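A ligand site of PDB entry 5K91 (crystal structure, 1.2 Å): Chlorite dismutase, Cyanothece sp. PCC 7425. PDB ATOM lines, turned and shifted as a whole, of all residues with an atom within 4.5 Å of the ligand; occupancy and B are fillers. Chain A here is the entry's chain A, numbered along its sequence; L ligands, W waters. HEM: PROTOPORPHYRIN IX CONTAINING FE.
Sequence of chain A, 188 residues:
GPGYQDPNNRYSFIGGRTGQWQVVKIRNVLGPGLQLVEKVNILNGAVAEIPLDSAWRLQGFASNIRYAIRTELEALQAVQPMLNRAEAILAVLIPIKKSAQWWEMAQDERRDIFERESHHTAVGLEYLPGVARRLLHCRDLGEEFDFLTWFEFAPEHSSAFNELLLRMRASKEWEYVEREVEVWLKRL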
ATOM      1  N   ASN A  64     -19.115   5.949 -10.666  1.00  0.00           N
ATOM      2  CA  ASN A  64     -18.237   7.095 -10.617  1.00  0.00           C
ATOM      3  C   ASN A  64     -17.410   7.255 -11.871  1.00  0.00           C
ATOM      4  O   ASN A  64     -17.227   6.352 -12.663  1.00  0.00           O
ATOM      5  CB  ASN A  64     -17.241   7.075  -9.431  1.00  0.00           C
ATOM      6  CG  ASN A  64     -16.219   5.959  -9.503  1.00  0.00           C
ATOM      7  OD1 ASN A  64     -16.766   4.834  -9.169  1.00  0.00           O
ATOM      8  ND2 ASN A  64     -15.017   6.105  -9.895  1.00  0.00           N
ATOM      9  N   ILE A  65     -16.910   8.481 -12.068  1.00  0.00           N
ATOM     10  CA  ILE A  65     -15.995   8.921 -13.163  1.00  0.00           C
ATOM     11  C   ILE A  65     -14.733   8.062 -13.086  1.00  0.00           C
ATOM     12  O   ILE A  65     -14.132   7.944 -12.024  1.00  0.00           O
ATOM     13  CB  ILE A  65     -15.759  10.467 -13.141  1.00  0.00           C
ATOM     14  CG1 ILE A  65     -17.054  11.167 -13.623  1.00  0.00           C
ATOM     15  CG2 ILE A  65     -14.595  10.794 -13.977  1.00  0.00           C
ATOM     16  CD1 ILE A  65     -17.488  10.955 -14.995  1.00  0.00           C
ATOM     17  N   ARG A  66     -14.280   7.608 -14.280  1.00  0.00           N
ATOM     18  CA  ARG A  66     -13.081   6.809 -14.487  1.00  0.00           C
ATOM     19  C   ARG A  66     -11.938   7.490 -15.185  1.00  0.00           C
ATOM     20  O   ARG A  66     -10.782   7.056 -14.965  1.00  0.00           O
ATOM     21  CB  ARG A  66     -13.591   5.401 -15.067  1.00  0.00           C
ATOM     22  CG  ARG A  66     -14.692   4.715 -14.516  1.00  0.00           C
ATOM     23  CD  ARG A  66     -14.325   4.916 -13.178  1.00  0.00           C
ATOM     24  NE  ARG A  66     -15.332   4.065 -12.744  1.00  0.00           N
ATOM     25  CZ  ARG A  66     -15.736   2.760 -12.734  1.00  0.00           C
ATOM     26  NH1 ARG A  66     -14.866   1.766 -13.313  1.00  0.00           N
ATOM     27  NH2 ARG A  66     -16.798   1.821 -12.332  1.00  0.00           N
ATOM     28  N   TYR A  67     -12.139   8.579 -16.000  1.00  0.00           N
ATOM     29  CA  TYR A  67     -11.175   9.184 -16.900  1.00  0.00           C
ATOM     30  C   TYR A  67     -11.218  10.677 -16.881  1.00  0.00           C
ATOM     31  O   TYR A  67     -10.173  11.306 -16.896  1.00  0.00           O
ATOM     32  CB  TYR A  67     -11.331   8.593 -18.288  1.00  0.00           C
ATOM     33  CG  TYR A  67     -10.995   7.122 -18.389  1.00  0.00           C
ATOM     34  CD1 TYR A  67      -9.724   6.614 -18.126  1.00  0.00           C
ATOM     35  CD2 TYR A  67     -11.958   6.241 -18.749  1.00  0.00           C
ATOM     36  CE1 TYR A  67      -9.441   5.303 -18.170  1.00  0.00           C
ATOM     37  CE2 TYR A  67     -11.735   4.887 -18.758  1.00  0.00           C
ATOM     38  CZ  TYR A  67     -10.423   4.467 -18.464  1.00  0.00           C
ATOM     39  OH  TYR A  67     -10.149   3.077 -18.496  1.00  0.00           O
ATOM     40  N   ALA A  68     -12.469  11.178 -16.855  1.00  0.00           N
ATOM     41  CA  ALA A  68     -12.655  12.614 -17.042  1.00  0.00           C
ATOM     42  C   ALA A  68     -11.963  13.382 -15.934  1.00  0.00           C
ATOM     43  O   ALA A  68     -12.097  13.082 -14.741  1.00  0.00           O
ATOM     44  CB  ALA A  68     -14.133  12.971 -17.116  1.00  0.00           C
ATOM     45  N   LEU A  76     -18.268  19.712 -19.790  1.00  0.00           N
ATOM     46  CA  LEU A  76     -19.467  18.878 -19.984  1.00  0.00           C
ATOM     47  C   LEU A  76     -20.667  19.445 -19.248  1.00  0.00           C
ATOM     48  O   LEU A  76     -21.776  19.523 -19.801  1.00  0.00           O
ATOM     49  CB  LEU A  76     -19.186  17.423 -19.472  1.00  0.00           C
ATOM     50  CG  LEU A  76     -18.227  16.670 -20.390  1.00  0.00           C
ATOM     51  CD1 LEU A  76     -17.599  15.494 -19.662  1.00  0.00           C
ATOM     52  CD2 LEU A  76     -18.904  16.118 -21.603  1.00  0.00           C
ATOM     53  N   ILE A  94     -26.422   1.361 -27.125  1.00  0.00           N
ATOM     54  CA  ILE A  94     -25.227   0.764 -27.739  1.00  0.00           C
ATOM     55  C   ILE A  94     -24.402  -0.005 -26.701  1.00  0.00           C
ATOM     56  O   ILE A  94     -23.549   0.591 -26.018  1.00  0.00           O
ATOM     57  CB  ILE A  94     -24.377   1.825 -28.478  1.00  0.00           C
ATOM     58  CG1 ILE A  94     -25.228   2.692 -29.452  1.00  0.00           C
ATOM     59  CG2 ILE A  94     -23.225   1.169 -29.179  1.00  0.00           C
ATOM     60  CD1 ILE A  94     -24.470   3.783 -30.190  1.00  0.00           C
ATOM     61  N   ILE A  96     -21.343  -2.185 -25.614  1.00  0.00           N
ATOM     62  CA  ILE A  96     -19.952  -2.235 -26.023  1.00  0.00           C
ATOM     63  C   ILE A  96     -19.155  -3.194 -25.177  1.00  0.00           C
ATOM     64  O   ILE A  96     -19.321  -3.193 -23.954  1.00  0.00           O
ATOM     65  CB  ILE A  96     -19.335  -0.836 -25.945  1.00  0.00           C
ATOM     66  CG1 ILE A  96     -19.996   0.025 -27.031  1.00  0.00           C
ATOM     67  CG2 ILE A  96     -17.828  -0.854 -26.083  1.00  0.00           C
ATOM     68  CD1 ILE A  96     -19.856   1.290 -26.905  1.00  0.00           C
ATOM     69  N   LYS A  98     -15.029  -4.269 -24.642  1.00  0.00           N
ATOM     70  CA  LYS A  98     -13.637  -4.013 -24.933  1.00  0.00           C
ATOM     71  C   LYS A  98     -12.803  -5.280 -24.650  1.00  0.00           C
ATOM     72  O   LYS A  98     -13.180  -6.170 -23.910  1.00  0.00           O
ATOM     73  CB  LYS A  98     -13.081  -2.830 -24.151  1.00  0.00           C
ATOM     74  CG  LYS A  98     -13.713  -1.507 -24.594  1.00  0.00           C
ATOM     75  CD  LYS A  98     -13.050  -0.366 -23.894  1.00  0.00           C
ATOM     76  CE  LYS A  98     -13.587   0.975 -24.423  1.00  0.00           C
ATOM     77  NZ  LYS A  98     -12.902   2.173 -23.856  1.00  0.00           N
ATOM     78  N   TRP A 102      -7.239  -4.339 -23.454  1.00  0.00           N
ATOM     79  CA  TRP A 102      -7.593  -3.047 -22.859  1.00  0.00           C
ATOM     80  C   TRP A 102      -7.605  -3.134 -21.353  1.00  0.00           C
ATOM     81  O   TRP A 102      -7.011  -2.327 -20.667  1.00  0.00           O
ATOM     82  CB  TRP A 102      -8.969  -2.641 -23.373  1.00  0.00           C
ATOM     83  CG  TRP A 102      -9.568  -1.456 -22.688  1.00  0.00           C
ATOM     84  CD1 TRP A 102     -10.451  -1.458 -21.629  1.00  0.00           C
ATOM     85  CD2 TRP A 102      -9.204  -0.082 -22.919  1.00  0.00           C
ATOM     86  NE1 TRP A 102     -10.690  -0.168 -21.253  1.00  0.00           N
ATOM     87  CE2 TRP A 102      -9.967   0.709 -22.043  1.00  0.00           C
ATOM     88  CE3 TRP A 102      -8.387   0.546 -23.842  1.00  0.00           C
ATOM     89  CZ2 TRP A 102      -9.893   2.083 -22.070  1.00  0.00           C
ATOM     90  CZ3 TRP A 102      -8.305   1.909 -23.820  1.00  0.00           C
ATOM     91  CH2 TRP A 102      -9.024   2.645 -22.960  1.00  0.00           C
ATOM     92  N   PHE A 114      -7.782   6.886 -24.336  1.00  0.00           N
ATOM     93  CA  PHE A 114      -9.115   7.479 -24.324  1.00  0.00           C
ATOM     94  C   PHE A 114      -9.124   8.939 -24.715  1.00  0.00           C
ATOM     95  O   PHE A 114      -9.980   9.330 -25.525  1.00  0.00           O
ATOM     96  CB  PHE A 114      -9.656   7.251 -22.882  1.00  0.00           C
ATOM     97  CG  PHE A 114     -11.061   7.793 -22.658  1.00  0.00           C
ATOM     98  CD1 PHE A 114     -12.180   7.063 -23.065  1.00  0.00           C
ATOM     99  CD2 PHE A 114     -11.270   8.998 -22.045  1.00  0.00           C
ATOM    100  CE1 PHE A 114     -13.487   7.522 -22.840  1.00  0.00           C
ATOM    101  CE2 PHE A 114     -12.586   9.494 -21.935  1.00  0.00           C
ATOM    102  CZ  PHE A 114     -13.669   8.697 -22.277  1.00  0.00           C
ATOM    103  N   HIS A 120     -11.734  11.461 -26.941  1.00  0.00           N
ATOM    104  CA  HIS A 120     -13.140  11.011 -26.763  1.00  0.00           C
ATOM    105  C   HIS A 120     -14.060  12.118 -26.304  1.00  0.00           C
ATOM    106  O   HIS A 120     -15.133  12.350 -26.889  1.00  0.00           O
ATOM    107  CB  HIS A 120     -13.287   9.825 -25.762  1.00  0.00           C
ATOM    108  CG  HIS A 120     -14.682   9.127 -25.672  1.00  0.00           C
ATOM    109  ND1 HIS A 120     -14.823   7.781 -25.949  1.00  0.00           N
ATOM    110  CD2 HIS A 120     -15.944   9.443 -25.149  1.00  0.00           C
ATOM    111  CE1 HIS A 120     -16.042   7.337 -25.658  1.00  0.00           C
ATOM    112  NE2 HIS A 120     -16.793   8.352 -25.263  1.00  0.00           N
ATOM    113  N   THR A 121     -13.703  12.774 -25.200  1.00  0.00           N
ATOM    114  CA  THR A 121     -14.588  13.772 -24.613  1.00  0.00           C
ATOM    115  C   THR A 121     -14.643  14.991 -25.515  1.00  0.00           C
ATOM    116  O   THR A 121     -15.694  15.598 -25.748  1.00  0.00           O
ATOM    117  CB  THR A 121     -14.048  14.167 -23.268  1.00  0.00           C
ATOM    118  OG1 THR A 121     -14.143  12.995 -22.422  1.00  0.00           O
ATOM    119  CG2 THR A 121     -14.880  15.273 -22.691  1.00  0.00           C
ATOM    120  N   GLY A 124     -16.935  14.129 -28.395  1.00  0.00           N
ATOM    121  CA  GLY A 124     -18.310  14.069 -28.025  1.00  0.00           C
ATOM    122  C   GLY A 124     -18.901  15.400 -27.677  1.00  0.00           C
ATOM    123  O   GLY A 124     -20.035  15.662 -28.007  1.00  0.00           O
ATOM    124  N   LEU A 125     -18.079  16.323 -27.119  1.00  0.00           N
ATOM    125  CA  LEU A 125     -18.568  17.652 -26.795  1.00  0.00           C
ATOM    126  C   LEU A 125     -19.104  18.379 -28.029  1.00  0.00           C
ATOM    127  O   LEU A 125     -19.959  19.237 -27.904  1.00  0.00           O
ATOM    128  CB  LEU A 125     -17.448  18.498 -26.175  1.00  0.00           C
ATOM    129  CG  LEU A 125     -17.327  18.384 -24.656  1.00  0.00           C
ATOM    130  CD1 LEU A 125     -15.975  18.891 -24.140  1.00  0.00           C
ATOM    131  CD2 LEU A 125     -18.432  19.151 -23.977  1.00  0.00           C
ATOM    132  N   LEU A 128     -22.930  18.152 -28.337  1.00  0.00           N
ATOM    133  CA  LEU A 128     -23.765  18.710 -27.279  1.00  0.00           C
ATOM    134  C   LEU A 128     -24.041  20.167 -27.627  1.00  0.00           C
ATOM    135  O   LEU A 128     -23.155  20.823 -28.173  1.00  0.00           O
ATOM    136  CB  LEU A 128     -23.060  18.587 -25.910  1.00  0.00           C
ATOM    137  CG  LEU A 128     -23.162  17.210 -25.183  1.00  0.00           C
ATOM    138  CD1 LEU A 128     -22.955  16.008 -26.126  1.00  0.00           C
ATOM    139  CD2 LEU A 128     -22.149  17.224 -24.021  1.00  0.00           C
ATOM    140  N   VAL A 131     -27.235  15.996 -28.160  1.00  0.00           N
ATOM    141  CA  VAL A 131     -27.274  14.598 -27.703  1.00  0.00           C
ATOM    142  C   VAL A 131     -27.132  14.524 -26.178  1.00  0.00           C
ATOM    143  O   VAL A 131     -26.155  15.028 -25.618  1.00  0.00           O
ATOM    144  CB  VAL A 131     -26.191  13.740 -28.399  1.00  0.00           C
ATOM    145  CG1 VAL A 131     -26.207  12.282 -27.902  1.00  0.00           C
ATOM    146  CG2 VAL A 131     -26.352  13.796 -29.951  1.00  0.00           C
ATOM    147  N   ARG A 133     -26.932  11.749 -22.879  1.00  0.00           N
ATOM    148  CA  ARG A 133     -26.302  10.429 -22.768  1.00  0.00           C
ATOM    149  C   ARG A 133     -26.384   9.936 -21.353  1.00  0.00           C
ATOM    150  O   ARG A 133     -26.537  10.686 -20.392  1.00  0.00           O
ATOM    151  CB  ARG A 133     -24.822  10.476 -23.189  1.00  0.00           C
ATOM    152  CG  ARG A 133     -23.918  11.185 -22.222  1.00  0.00           C
ATOM    153  CD  ARG A 133     -22.515  11.570 -22.799  1.00  0.00           C
ATOM    154  NE  ARG A 133     -21.625  11.978 -21.745  1.00  0.00           N
ATOM    155  CZ  ARG A 133     -21.673  13.143 -21.110  1.00  0.00           C
ATOM    156  NH1 ARG A 133     -22.402  14.130 -21.578  1.00  0.00           N
ATOM    157  NH2 ARG A 133     -20.924  13.393 -20.033  1.00  0.00           N
ATOM    158  N   LEU A 135     -24.086   6.686 -19.285  1.00  0.00           N
ATOM    159  CA  LEU A 135     -23.089   5.617 -19.305  1.00  0.00           C
ATOM    160  C   LEU A 135     -23.385   4.593 -18.203  1.00  0.00           C
ATOM    161  O   LEU A 135     -23.481   4.999 -17.031  1.00  0.00           O
ATOM    162  CB  LEU A 135     -21.698   6.208 -19.162  1.00  0.00           C
ATOM    163  CG  LEU A 135     -20.615   5.130 -19.049  1.00  0.00           C
ATOM    164  CD1 LEU A 135     -20.429   4.261 -20.294  1.00  0.00           C
ATOM    165  CD2 LEU A 135     -19.328   5.746 -18.718  1.00  0.00           C
ATOM    166  N   PHE A 147     -20.155  -2.252 -21.211  1.00  0.00           N
ATOM    167  CA  PHE A 147     -20.773  -0.937 -21.100  1.00  0.00           C
ATOM    168  C   PHE A 147     -22.159  -1.086 -21.755  1.00  0.00           C
ATOM    169  O   PHE A 147     -22.302  -1.737 -22.797  1.00  0.00           O
ATOM    170  CB  PHE A 147     -19.955   0.264 -21.629  1.00  0.00           C
ATOM    171  CG  PHE A 147     -18.629   0.264 -21.112  1.00  0.00           C
ATOM    172  CD1 PHE A 147     -18.275   0.855 -19.925  1.00  0.00           C
ATOM    173  CD2 PHE A 147     -17.631  -0.228 -21.867  1.00  0.00           C
ATOM    174  CE1 PHE A 147     -17.012   0.863 -19.472  1.00  0.00           C
ATOM    175  CE2 PHE A 147     -16.327  -0.175 -21.463  1.00  0.00           C
ATOM    176  CZ  PHE A 147     -16.000   0.392 -20.301  1.00  0.00           C
ATOM    177  N   THR A 149     -24.270   2.018 -23.313  1.00  0.00           N
ATOM    178  CA  THR A 149     -24.325   3.445 -23.539  1.00  0.00           C
ATOM    179  C   THR A 149     -25.663   3.777 -24.094  1.00  0.00           C
ATOM    180  O   THR A 149     -26.245   3.049 -24.880  1.00  0.00           O
ATOM    181  CB  THR A 149     -23.155   3.845 -24.419  1.00  0.00           C
ATOM    182  OG1 THR A 149     -23.272   3.337 -25.752  1.00  0.00           O
ATOM    183  CG2 THR A 149     -21.852   3.410 -23.822  1.00  0.00           C
ATOM    184  N   PHE A 151     -28.132   7.021 -25.594  1.00  0.00           N
ATOM    185  CA  PHE A 151     -28.129   8.362 -26.204  1.00  0.00           C
ATOM    186  C   PHE A 151     -29.533   8.739 -26.576  1.00  0.00           C
ATOM    187  O   PHE A 151     -30.273   7.882 -27.024  1.00  0.00           O
ATOM    188  CB  PHE A 151     -27.205   8.426 -27.452  1.00  0.00           C
ATOM    189  CG  PHE A 151     -25.811   8.008 -27.052  1.00  0.00           C
ATOM    190  CD1 PHE A 151     -24.879   8.894 -26.598  1.00  0.00           C
ATOM    191  CD2 PHE A 151     -25.447   6.728 -27.245  1.00  0.00           C
ATOM    192  CE1 PHE A 151     -23.679   8.413 -26.123  1.00  0.00           C
ATOM    193  CE2 PHE A 151     -24.212   6.282 -26.825  1.00  0.00           C
ATOM    194  CZ  PHE A 151     -23.345   7.090 -26.311  1.00  0.00           C
ATOM    195  N   PHE A 161     -25.515  12.409 -35.129  1.00  0.00           N
ATOM    196  CA  PHE A 161     -25.177  11.300 -34.271  1.00  0.00           C
ATOM    197  C   PHE A 161     -24.541  10.189 -35.083  1.00  0.00           C
ATOM    198  O   PHE A 161     -23.576   9.566 -34.633  1.00  0.00           O
ATOM    199  CB  PHE A 161     -26.400  10.859 -33.510  1.00  0.00           C
ATOM    200  CG  PHE A 161     -26.066   9.796 -32.530  1.00  0.00           C
ATOM    201  CD1 PHE A 161     -25.477  10.132 -31.330  1.00  0.00           C
ATOM    202  CD2 PHE A 161     -26.361   8.453 -32.768  1.00  0.00           C
ATOM    203  CE1 PHE A 161     -25.160   9.127 -30.377  1.00  0.00           C
ATOM    204  CE2 PHE A 161     -26.013   7.470 -31.832  1.00  0.00           C
ATOM    205  CZ  PHE A 161     -25.386   7.817 -30.655  1.00  0.00           C
ATOM    206  N   LEU A 164     -20.972  11.065 -35.545  1.00  0.00           N
ATOM    207  CA  LEU A 164     -20.213  10.813 -34.322  1.00  0.00           C
ATOM    208  C   LEU A 164     -19.850   9.338 -34.200  1.00  0.00           C
ATOM    209  O   LEU A 164     -18.726   9.017 -33.846  1.00  0.00           O
ATOM    210  CB  LEU A 164     -21.058  11.242 -33.120  1.00  0.00           C
ATOM    211  CG  LEU A 164     -20.499  10.844 -31.764  1.00  0.00           C
ATOM    212  CD1 LEU A 164     -19.150  11.465 -31.485  1.00  0.00           C
ATOM    213  CD2 LEU A 164     -21.555  11.277 -30.726  1.00  0.00           C
ATOM    214  N   LEU A 165     -20.801   8.442 -34.464  1.00  0.00           N
ATOM    215  CA  LEU A 165     -20.492   7.024 -34.360  1.00  0.00           C
ATOM    216  C   LEU A 165     -19.321   6.644 -35.258  1.00  0.00           C
ATOM    217  O   LEU A 165     -18.426   5.921 -34.836  1.00  0.00           O
ATOM    218  CB  LEU A 165     -21.700   6.188 -34.740  1.00  0.00           C
ATOM    219  CG  LEU A 165     -22.918   6.245 -33.792  1.00  0.00           C
ATOM    220  CD1 LEU A 165     -23.977   5.399 -34.385  1.00  0.00           C
ATOM    221  CD2 LEU A 165     -22.534   5.776 -32.411  1.00  0.00           C
ATOM    222  N   MET A 168     -16.010   7.983 -33.853  1.00  0.00           N
ATOM    223  CA  MET A 168     -15.513   7.165 -32.746  1.00  0.00           C
ATOM    224  C   MET A 168     -14.926   5.866 -33.251  1.00  0.00           C
ATOM    225  O   MET A 168     -13.868   5.413 -32.768  1.00  0.00           O
ATOM    226  CB  MET A 168     -16.644   6.936 -31.731  1.00  0.00           C
ATOM    227  CG  MET A 168     -17.071   8.279 -31.242  1.00  0.00           C
ATOM    228  SD  MET A 168     -18.062   8.328 -29.798  1.00  0.00           S
ATOM    229  CE  MET A 168     -17.101   9.583 -28.934  1.00  0.00           C
ATOM    230  N   GLU A 173      -9.067   4.284 -29.515  1.00  0.00           N
ATOM    231  CA  GLU A 173      -9.866   3.551 -28.511  1.00  0.00           C
ATOM    232  C   GLU A 173     -10.629   2.411 -29.133  1.00  0.00           C
ATOM    233  O   GLU A 173     -10.783   1.321 -28.536  1.00  0.00           O
ATOM    234  CB  GLU A 173     -10.825   4.545 -27.819  1.00  0.00           C
ATOM    235  CG  GLU A 173     -11.725   3.932 -26.712  1.00  0.00           C
ATOM    236  CD  GLU A 173     -12.667   4.910 -26.198  1.00  0.00           C
ATOM    237  OE1 GLU A 173     -12.870   6.023 -26.706  1.00  0.00           O
ATOM    238  OE2 GLU A 173     -13.329   4.517 -25.210  1.00  0.00           O
ATOM    239  N   TRP A 174     -11.201   2.644 -30.318  1.00  0.00           N
ATOM    240  CA  TRP A 174     -12.033   1.651 -30.934  1.00  0.00           C
ATOM    241  C   TRP A 174     -11.270   0.445 -31.485  1.00  0.00           C
ATOM    242  O   TRP A 174     -11.869  -0.593 -31.742  1.00  0.00           O
ATOM    243  CB  TRP A 174     -12.921   2.224 -32.024  1.00  0.00           C
ATOM    244  CG  TRP A 174     -14.400   2.177 -31.603  1.00  0.00           C
ATOM    245  CD1 TRP A 174     -15.368   1.337 -32.047  1.00  0.00           C
ATOM    246  CD2 TRP A 174     -14.995   2.952 -30.562  1.00  0.00           C
ATOM    247  NE1 TRP A 174     -16.559   1.562 -31.400  1.00  0.00           N
ATOM    248  CE2 TRP A 174     -16.358   2.569 -30.509  1.00  0.00           C
ATOM    249  CE3 TRP A 174     -14.568   3.925 -29.734  1.00  0.00           C
ATOM    250  CZ2 TRP A 174     -17.279   3.099 -29.599  1.00  0.00           C
ATOM    251  CZ3 TRP A 174     -15.473   4.515 -28.827  1.00  0.00           C
ATOM    252  CH2 TRP A 174     -16.837   4.118 -28.768  1.00  0.00           C
ATOM    253  N   GLU A 180     -20.052  -4.661 -30.512  1.00  0.00           N
ATOM    254  CA  GLU A 180     -20.828  -3.442 -30.539  1.00  0.00           C
ATOM    255  C   GLU A 180     -22.138  -3.709 -31.277  1.00  0.00           C
ATOM    256  O   GLU A 180     -22.118  -4.310 -32.359  1.00  0.00           O
ATOM    257  CB  GLU A 180     -20.034  -2.328 -31.273  1.00  0.00           C
ATOM    258  CG  GLU A 180     -20.766  -0.974 -31.354  1.00  0.00           C
ATOM    259  CD  GLU A 180     -19.872   0.168 -31.883  1.00  0.00           C
ATOM    260  OE1 GLU A 180     -18.723  -0.069 -32.331  1.00  0.00           O
ATOM    261  OE2 GLU A 180     -20.353   1.322 -31.821  1.00  0.00           O
HETATM  262  CHA HEM L   1     -17.155   7.145 -21.653  1.00  0.00           C
HETATM  263  CHB HEM L   1     -18.372  11.594 -23.128  1.00  0.00           C
HETATM  264  CHC HEM L   1     -20.501   9.692 -26.994  1.00  0.00           C
HETATM  265  CHD HEM L   1     -19.092   5.254 -25.572  1.00  0.00           C
HETATM  266  C1A HEM L   1     -17.316   8.478 -21.684  1.00  0.00           C
HETATM  267  C2A HEM L   1     -16.721   9.502 -20.764  1.00  0.00           C
HETATM  268  C3A HEM L   1     -17.097  10.749 -21.149  1.00  0.00           C
HETATM  269  C4A HEM L   1     -17.842  10.624 -22.313  1.00  0.00           C
HETATM  270  CMA HEM L   1     -16.851  12.078 -20.504  1.00  0.00           C
HETATM  271  CAA HEM L   1     -15.857   9.096 -19.541  1.00  0.00           C
HETATM  272  CBA HEM L   1     -16.688   8.931 -18.317  1.00  0.00           C
HETATM  273  CGA HEM L   1     -15.684   8.641 -17.199  1.00  0.00           C
HETATM  274  O1A HEM L   1     -15.884   7.614 -16.481  1.00  0.00           O
HETATM  275  O2A HEM L   1     -14.711   9.318 -16.990  1.00  0.00           O
HETATM  276  C1B HEM L   1     -19.092  11.399 -24.271  1.00  0.00           C
HETATM  277  C2B HEM L   1     -19.834  12.408 -24.958  1.00  0.00           C
HETATM  278  C3B HEM L   1     -20.481  11.933 -25.971  1.00  0.00           C
HETATM  279  C4B HEM L   1     -20.193  10.559 -25.999  1.00  0.00           C
HETATM  280  CMB HEM L   1     -19.872  13.835 -24.503  1.00  0.00           C
HETATM  281  CAB HEM L   1     -21.421  12.711 -26.915  1.00  0.00           C
HETATM  282  CBB HEM L   1     -22.542  12.197 -27.395  1.00  0.00           C
HETATM  283  C1C HEM L   1     -20.255   8.353 -27.019  1.00  0.00           C
HETATM  284  C2C HEM L   1     -20.656   7.404 -28.021  1.00  0.00           C
HETATM  285  C3C HEM L   1     -20.316   6.156 -27.627  1.00  0.00           C
HETATM  286  C4C HEM L   1     -19.645   6.286 -26.373  1.00  0.00           C
HETATM  287  CMC HEM L   1     -21.512   7.681 -29.273  1.00  0.00           C
HETATM  288  CAC HEM L   1     -20.610   4.843 -28.294  1.00  0.00           C
HETATM  289  CBC HEM L   1     -20.565   4.575 -29.565  1.00  0.00           C
HETATM  290  C1D HEM L   1     -18.482   5.486 -24.324  1.00  0.00           C
HETATM  291  C2D HEM L   1     -17.888   4.364 -23.601  1.00  0.00           C
HETATM  292  C3D HEM L   1     -17.420   4.886 -22.505  1.00  0.00           C
HETATM  293  C4D HEM L   1     -17.567   6.325 -22.592  1.00  0.00           C
HETATM  294  CMD HEM L   1     -17.911   2.928 -24.014  1.00  0.00           C
HETATM  295  CAD HEM L   1     -16.640   4.173 -21.363  1.00  0.00           C
HETATM  296  CBD HEM L   1     -15.140   4.111 -21.658  1.00  0.00           C
HETATM  297  CGD HEM L   1     -14.304   3.295 -20.674  1.00  0.00           C
HETATM  298  O1D HEM L   1     -14.609   3.341 -19.473  1.00  0.00           O
HETATM  299  O2D HEM L   1     -13.430   2.514 -21.171  1.00  0.00           O
HETATM  300  NA  HEM L   1     -17.956   9.290 -22.648  1.00  0.00           N
HETATM  301  NB  HEM L   1     -19.336  10.237 -24.978  1.00  0.00           N
HETATM  302  NC  HEM L   1     -19.607   7.645 -26.046  1.00  0.00           N
HETATM  303  ND  HEM L   1     -18.360   6.695 -23.671  1.00  0.00           N
HETATM  304 FE   HEM L   1     -18.640   8.418 -24.422  1.00  0.00          FE
HETATM  305  O   HOH W   1     -18.152   6.422 -15.311  1.00  0.00           O
HETATM  306  O   HOH W   2     -20.400   9.549 -20.576  1.00  0.00           O
HETATM  307  O   HOH W   3     -11.992   1.413 -19.240  1.00  0.00           O
HETATM  308  O   HOH W   4     -13.883   1.790 -17.190  1.00  0.00           O
HETATM  309  O   HOH W   5     -15.976   4.883 -17.668  1.00  0.00           O
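The backbone carbonyl oxygen (O) of Phe 114 is in hydrogen-bond range of the backbone NH (N) of His 120 (3.1 Å).
ND1 of His 120 is in hydrogen-bond range of OE1 of Glu 173, 2.7 Å away.
NE of Arg 66 lies within hydrogen-bond range of O of Asn 64 (3.0 Å).
The side-chain carboxylate of Glu 173 is in salt-bridge range of the side-chain amino group of Lys 98, at 2.7 Å.
The backbone carbonyl oxygen (O) of Phe 147 sits at hydrogen-bond distance from the backbone NH (N) of Ile 96, 3.0 Å away.
The side-chain carboxylate of Glu 180 sits at hydrogen-bond distance from the indole nitrogen of Trp 174, at 2.9 Å.
OG1 of Thr 149 is in hydrogen-bond range of O of Ile 94 (2.8 Å).
Residues that only touch the ligand: Phe 151 (3.2 Å), Met 168 (3.3 Å), Ile 65 (3.4 Å), Phe 147 (3.4 Å), Gly 124 (3.4 Å), Thr 121 (3.4 Å), Phe 114 (3.5 Å), Arg 133 (3.5 Å), Leu 164 (3.6 Å), Leu 76 (3.6 Å), Trp 174 (3.6 Å), Leu 165 (3.7 Å), Trp 102 (3.7 Å), Val 131 (3.7 Å), Leu 128 (3.7 Å), Thr 149 (3.8 Å), Leu 135 (3.8 Å), Ile 96 (3.9 Å) and Glu 180 (3.96 Å).
Hydrophobic or aromatic side chains that line the ligand: Ile 65, Tyr 67, Ala 68, Leu 76, Ile 96, Trp 102, Phe 114, His 120, Leu 128, Val 131, Leu 135, Phe 147, Phe 151, Leu 164, Leu 165, Met 168 and Trp 174.
24 residues have an atom within 4 Å of the ligand: Ile 65, Arg 66, Tyr 67, Ala 68, Leu 76, Ile 96, Lys 98, Trp 102, Phe 114, His 120, Thr 121, Gly 124, Leu 128, Val 131, Arg 133, Leu 135, Phe 147, Thr 149, Phe 151, Leu 164, Leu 165, Met 168, Trp 174 and Glu 180.
Water W3 lies within hydrogen-bond range of OH of Tyr 67 (2.6 Å), O2D of the ligand (2.6 Å) and NE1 of Trp 102 (2.9 Å).
Water W1 lies within hydrogen-bond range of O of Asn 64 and O1A of the ligand.
A ring nitrogen (NE2) of His 120 binds an iron atom (FE) of the ligand, at 2.0 Å.
The backbone NH (N) of Arg 66 lies within hydrogen-bond range of an oxygen (O1A) of the ligand, 2.7 Å away.
O2D of the ligand lies within salt-bridge range of NZ of Lys 98.
An oxygen (O2A) of the ligand is in hydrogen-bond range of the backbone NH (N) of Tyr 67 (2.9 Å).
The backbone NH of Ala 68 lies within hydrogen-bond range of an oxygen (O2A) of the ligand, at 2.9 Å.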
